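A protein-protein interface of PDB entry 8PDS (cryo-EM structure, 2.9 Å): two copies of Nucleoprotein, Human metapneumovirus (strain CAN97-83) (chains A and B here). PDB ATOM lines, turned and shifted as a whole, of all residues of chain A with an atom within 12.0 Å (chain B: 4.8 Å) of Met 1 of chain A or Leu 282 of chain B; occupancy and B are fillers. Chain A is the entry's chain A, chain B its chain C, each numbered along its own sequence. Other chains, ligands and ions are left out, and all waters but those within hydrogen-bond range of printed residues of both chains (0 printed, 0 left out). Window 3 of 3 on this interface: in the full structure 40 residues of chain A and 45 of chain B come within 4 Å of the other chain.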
ATOM      1  N   MET A   1     -20.081 -12.690 -18.469  1.00  0.00           N
ATOM      2  CA  MET A   1     -21.275 -11.860 -18.575  1.00  0.00           C
ATOM      3  C   MET A   1     -22.149 -12.298 -19.746  1.00  0.00           C
ATOM      4  O   MET A   1     -23.137 -13.007 -19.563  1.00  0.00           O
ATOM      5  CB  MET A   1     -20.891 -10.387 -18.726  1.00  0.00           C
ATOM      6  CG  MET A   1     -22.073  -9.431 -18.724  1.00  0.00           C
ATOM      7  SD  MET A   1     -22.975  -9.437 -17.163  1.00  0.00           S
ATOM      8  CE  MET A   1     -21.817  -8.577 -16.101  1.00  0.00           C
ATOM      9  N   SER A   2     -21.776 -11.874 -20.950  1.00  0.00           N
ATOM     10  CA  SER A   2     -22.530 -12.179 -22.155  1.00  0.00           C
ATOM     11  C   SER A   2     -21.857 -13.295 -22.942  1.00  0.00           C
ATOM     12  O   SER A   2     -20.631 -13.443 -22.928  1.00  0.00           O
ATOM     13  CB  SER A   2     -22.674 -10.940 -23.040  1.00  0.00           C
ATOM     14  OG  SER A   2     -21.438 -10.602 -23.644  1.00  0.00           O
ATOM     15  N   LEU A   3     -22.677 -14.084 -23.628  1.00  0.00           N
ATOM     16  CA  LEU A   3     -22.198 -15.159 -24.496  1.00  0.00           C
ATOM     17  C   LEU A   3     -22.016 -14.659 -25.923  1.00  0.00           C
ATOM     18  O   LEU A   3     -22.498 -15.264 -26.874  1.00  0.00           O
ATOM     19  CB  LEU A   3     -23.180 -16.321 -24.460  1.00  0.00           C
ATOM     20  CG  LEU A   3     -23.740 -16.777 -23.115  1.00  0.00           C
ATOM     21  CD1 LEU A   3     -24.930 -17.688 -23.343  1.00  0.00           C
ATOM     22  CD2 LEU A   3     -22.692 -17.480 -22.296  1.00  0.00           C
ATOM     23  N   GLN A   4     -21.315 -13.542 -26.088  1.00  0.00           N
ATOM     24  CA  GLN A   4     -21.246 -12.883 -27.385  1.00  0.00           C
ATOM     25  C   GLN A   4     -20.008 -13.253 -28.185  1.00  0.00           C
ATOM     26  O   GLN A   4     -20.075 -13.315 -29.417  1.00  0.00           O
ATOM     27  CB  GLN A   4     -21.299 -11.362 -27.205  1.00  0.00           C
ATOM     28  CG  GLN A   4     -21.309 -10.582 -28.504  1.00  0.00           C
ATOM     29  CD  GLN A   4     -22.526 -10.890 -29.349  1.00  0.00           C
ATOM     30  OE1 GLN A   4     -22.438 -11.603 -30.347  1.00  0.00           O
ATOM     31  NE2 GLN A   4     -23.675 -10.355 -28.951  1.00  0.00           N
ATOM     32  N   GLY A   5     -18.887 -13.508 -27.520  1.00  0.00           N
ATOM     33  CA  GLY A   5     -17.686 -13.895 -28.226  1.00  0.00           C
ATOM     34  C   GLY A   5     -17.636 -15.339 -28.655  1.00  0.00           C
ATOM     35  O   GLY A   5     -16.698 -15.729 -29.353  1.00  0.00           O
ATOM     36  N   ILE A   6     -18.629 -16.137 -28.269  1.00  0.00           N
ATOM     37  CA  ILE A   6     -18.660 -17.553 -28.609  1.00  0.00           C
ATOM     38  C   ILE A   6     -19.164 -17.713 -30.036  1.00  0.00           C
ATOM     39  O   ILE A   6     -20.371 -17.812 -30.276  1.00  0.00           O
ATOM     40  CB  ILE A   6     -19.523 -18.340 -27.612  1.00  0.00           C
ATOM     41  CG1 ILE A   6     -18.991 -18.145 -26.196  1.00  0.00           C
ATOM     42  CG2 ILE A   6     -19.529 -19.809 -27.957  1.00  0.00           C
ATOM     43  CD1 ILE A   6     -19.783 -18.882 -25.151  1.00  0.00           C
ATOM     44  N   HIS A   7     -18.237 -17.736 -30.989  1.00  0.00           N
ATOM     45  CA  HIS A   7     -18.554 -17.791 -32.407  1.00  0.00           C
ATOM     46  C   HIS A   7     -17.367 -18.426 -33.115  1.00  0.00           C
ATOM     47  O   HIS A   7     -16.224 -18.213 -32.710  1.00  0.00           O
ATOM     48  CB  HIS A   7     -18.838 -16.388 -32.956  1.00  0.00           C
ATOM     49  CG  HIS A   7     -19.457 -16.380 -34.317  1.00  0.00           C
ATOM     50  ND1 HIS A   7     -18.903 -15.701 -35.381  1.00  0.00           N
ATOM     51  CD2 HIS A   7     -20.588 -16.957 -34.786  1.00  0.00           C
ATOM     52  CE1 HIS A   7     -19.663 -15.867 -36.449  1.00  0.00           C
ATOM     53  NE2 HIS A   7     -20.691 -16.625 -36.115  1.00  0.00           N
ATOM     54  N   LEU B 273     -25.268 -22.034 -18.420  1.00  0.00           N
ATOM     55  CA  LEU B 273     -24.247 -21.073 -18.816  1.00  0.00           C
ATOM     56  C   LEU B 273     -24.338 -19.802 -17.986  1.00  0.00           C
ATOM     57  O   LEU B 273     -23.331 -19.113 -17.792  1.00  0.00           O
ATOM     58  CB  LEU B 273     -24.387 -20.737 -20.300  1.00  0.00           C
ATOM     59  CG  LEU B 273     -23.954 -21.773 -21.336  1.00  0.00           C
ATOM     60  CD1 LEU B 273     -24.374 -21.314 -22.715  1.00  0.00           C
ATOM     61  CD2 LEU B 273     -22.457 -21.998 -21.293  1.00  0.00           C
ATOM     62  N   VAL B 278     -19.715 -20.117 -14.152  1.00  0.00           N
ATOM     63  CA  VAL B 278     -19.395 -19.999 -15.572  1.00  0.00           C
ATOM     64  C   VAL B 278     -19.265 -18.531 -15.966  1.00  0.00           C
ATOM     65  O   VAL B 278     -18.356 -18.152 -16.718  1.00  0.00           O
ATOM     66  CB  VAL B 278     -20.460 -20.730 -16.408  1.00  0.00           C
ATOM     67  CG1 VAL B 278     -20.006 -20.888 -17.838  1.00  0.00           C
ATOM     68  CG2 VAL B 278     -20.761 -22.080 -15.798  1.00  0.00           C
ATOM     69  N   GLN B 279     -20.160 -17.686 -15.442  1.00  0.00           N
ATOM     70  CA  GLN B 279     -20.135 -16.257 -15.736  1.00  0.00           C
ATOM     71  C   GLN B 279     -18.793 -15.636 -15.386  1.00  0.00           C
ATOM     72  O   GLN B 279     -18.356 -14.689 -16.049  1.00  0.00           O
ATOM     73  CB  GLN B 279     -21.252 -15.549 -14.968  1.00  0.00           C
ATOM     74  CG  GLN B 279     -22.656 -15.924 -15.410  1.00  0.00           C
ATOM     75  CD  GLN B 279     -23.044 -15.294 -16.729  1.00  0.00           C
ATOM     76  OE1 GLN B 279     -23.005 -15.940 -17.775  1.00  0.00           O
ATOM     77  NE2 GLN B 279     -23.442 -14.029 -16.685  1.00  0.00           N
ATOM     78  N   ALA B 280     -18.127 -16.148 -14.352  1.00  0.00           N
ATOM     79  CA  ALA B 280     -16.797 -15.669 -14.004  1.00  0.00           C
ATOM     80  C   ALA B 280     -15.739 -16.072 -15.021  1.00  0.00           C
ATOM     81  O   ALA B 280     -14.608 -15.585 -14.934  1.00  0.00           O
ATOM     82  CB  ALA B 280     -16.402 -16.184 -12.622  1.00  0.00           C
ATOM     83  N   GLU B 281     -16.069 -16.947 -15.970  1.00  0.00           N
ATOM     84  CA  GLU B 281     -15.114 -17.451 -16.942  1.00  0.00           C
ATOM     85  C   GLU B 281     -15.445 -17.090 -18.379  1.00  0.00           C
ATOM     86  O   GLU B 281     -14.604 -17.320 -19.258  1.00  0.00           O
ATOM     87  CB  GLU B 281     -15.007 -18.979 -16.837  1.00  0.00           C
ATOM     88  CG  GLU B 281     -14.707 -19.473 -15.440  1.00  0.00           C
ATOM     89  CD  GLU B 281     -14.819 -20.970 -15.324  1.00  0.00           C
ATOM     90  OE1 GLU B 281     -15.440 -21.579 -16.213  1.00  0.00           O
ATOM     91  OE2 GLU B 281     -14.293 -21.535 -14.345  1.00  0.00           O
ATOM     92  N   LEU B 282     -16.647 -16.578 -18.651  1.00  0.00           N
ATOM     93  CA  LEU B 282     -16.966 -16.216 -20.034  1.00  0.00           C
ATOM     94  C   LEU B 282     -15.990 -15.209 -20.623  1.00  0.00           C
ATOM     95  O   LEU B 282     -15.822 -15.169 -21.844  1.00  0.00           O
ATOM     96  CB  LEU B 282     -18.389 -15.679 -20.186  1.00  0.00           C
ATOM     97  CG  LEU B 282     -19.529 -16.677 -20.375  1.00  0.00           C
ATOM     98  CD1 LEU B 282     -19.283 -17.403 -21.683  1.00  0.00           C
ATOM     99  CD2 LEU B 282     -19.681 -17.660 -19.269  1.00  0.00           C
ATOM    100  N   LYS B 283     -15.336 -14.395 -19.800  1.00  0.00           N
ATOM    101  CA  LYS B 283     -14.360 -13.453 -20.343  1.00  0.00           C
ATOM    102  C   LYS B 283     -13.155 -14.172 -20.953  1.00  0.00           C
ATOM    103  O   LYS B 283     -12.740 -13.857 -22.075  1.00  0.00           O
ATOM    104  CB  LYS B 283     -13.957 -12.456 -19.256  1.00  0.00           C
ATOM    105  CG  LYS B 283     -13.226 -13.043 -18.069  1.00  0.00           C
ATOM    106  CD  LYS B 283     -12.851 -11.953 -17.087  1.00  0.00           C
ATOM    107  CE  LYS B 283     -14.081 -11.428 -16.356  1.00  0.00           C
ATOM    108  NZ  LYS B 283     -14.708 -12.446 -15.467  1.00  0.00           N
ATOM    109  N   GLN B 284     -12.614 -15.179 -20.267  1.00  0.00           N
ATOM    110  CA  GLN B 284     -11.505 -15.931 -20.845  1.00  0.00           C
ATOM    111  C   GLN B 284     -11.974 -16.863 -21.955  1.00  0.00           C
ATOM    112  O   GLN B 284     -11.217 -17.139 -22.893  1.00  0.00           O
ATOM    113  CB  GLN B 284     -10.779 -16.713 -19.756  1.00  0.00           C
ATOM    114  CG  GLN B 284      -9.955 -15.842 -18.826  1.00  0.00           C
ATOM    115  CD  GLN B 284      -8.904 -16.628 -18.081  1.00  0.00           C
ATOM    116  OE1 GLN B 284      -8.377 -17.616 -18.591  1.00  0.00           O
ATOM    117  NE2 GLN B 284      -8.595 -16.200 -16.863  1.00  0.00           N
ATOM    118  N   VAL B 285     -13.210 -17.350 -21.876  1.00  0.00           N
ATOM    119  CA  VAL B 285     -13.778 -18.110 -22.986  1.00  0.00           C
ATOM    120  C   VAL B 285     -13.818 -17.250 -24.246  1.00  0.00           C
ATOM    121  O   VAL B 285     -13.419 -17.676 -25.340  1.00  0.00           O
ATOM    122  CB  VAL B 285     -15.178 -18.626 -22.606  1.00  0.00           C
ATOM    123  CG1 VAL B 285     -15.871 -19.241 -23.799  1.00  0.00           C
ATOM    124  CG2 VAL B 285     -15.086 -19.616 -21.464  1.00  0.00           C
ATOM    125  N   THR B 286     -14.303 -16.017 -24.101  1.00  0.00           N
ATOM    126  CA  THR B 286     -14.331 -15.077 -25.208  1.00  0.00           C
ATOM    127  C   THR B 286     -12.928 -14.766 -25.699  1.00  0.00           C
ATOM    128  O   THR B 286     -12.727 -14.576 -26.898  1.00  0.00           O
ATOM    129  CB  THR B 286     -15.052 -13.798 -24.780  1.00  0.00           C
ATOM    130  OG1 THR B 286     -16.395 -14.114 -24.392  1.00  0.00           O
ATOM    131  CG2 THR B 286     -15.087 -12.788 -25.911  1.00  0.00           C
ATOM    132  N   PHE B 321     -17.073 -23.805 -17.242  1.00  0.00           N
ATOM    133  CA  PHE B 321     -17.584 -23.713 -18.604  1.00  0.00           C
ATOM    134  C   PHE B 321     -17.415 -25.036 -19.335  1.00  0.00           C
ATOM    135  O   PHE B 321     -18.305 -25.461 -20.078  1.00  0.00           O
ATOM    136  CB  PHE B 321     -16.881 -22.587 -19.357  1.00  0.00           C
ATOM    137  CG  PHE B 321     -17.273 -22.485 -20.805  1.00  0.00           C
ATOM    138  CD1 PHE B 321     -18.441 -21.851 -21.177  1.00  0.00           C
ATOM    139  CD2 PHE B 321     -16.463 -23.017 -21.793  1.00  0.00           C
ATOM    140  CE1 PHE B 321     -18.796 -21.753 -22.503  1.00  0.00           C
ATOM    141  CE2 PHE B 321     -16.814 -22.922 -23.119  1.00  0.00           C
ATOM    142  CZ  PHE B 321     -17.982 -22.289 -23.475  1.00  0.00           C
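The backbone carbonyl oxygen (O) of Met 1 of chain A sits at hydrogen-bond distance from the side-chain amide nitrogen (NE2) of Gln 279 of chain B (3.1 Å).
OE1 of Gln 279 of chain B sits close to O of Leu 273 of chain B (3.2 Å).
The backbone carbonyl oxygen (O) of Leu 282 of chain B sits at hydrogen-bond distance from the side-chain hydroxyl (OG1) of Thr 286 of chain B.
Met 1 of chain A touches Leu 282 of chain B.
Leu 3 of chain A touches Leu 273 of chain B.
Leu 3 of chain A touches Leu 282 of chain B.
Thr 286 of chain B touches Gly 5 of chain A (CG2 to CA, 3.7 Å).
CD1 of Leu 282 of chain B touches CD1 of Ile 6 of chain A, 3.8 Å away.
Met 1 of chain A touches two residues of chain B.
Printed residues of chain B within 4 Å of Leu 3 of chain A: Leu 273 and Leu 282.
Printed residues of chain B within 4 Å of Gly 5 of chain A: Thr 286 (3.7 Å).
Printed residues of chain B within 4 Å of Ile 6 of chain A: Leu 282 (3.8 Å).
Val 278 of chain B touches none of the printed residues of chain A.
Of chain A, only Met 1 comes within 4 Å of Gln 279 of chain B.
No residue of chain A comes within 4 Å of Ala 280 of chain B.
Leu 282 of chain B touches three residues of chain A.
No residue of chain A comes within 4 Å of Val 285 of chain B.
Among the printed residues, 6 pairs touch across the chains.
Among the printed residues, no Asp or Glu carboxylate lies within 4 Å of a Lys or Arg side-chain nitrogen of the other chain.
No position is printed for both chains.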
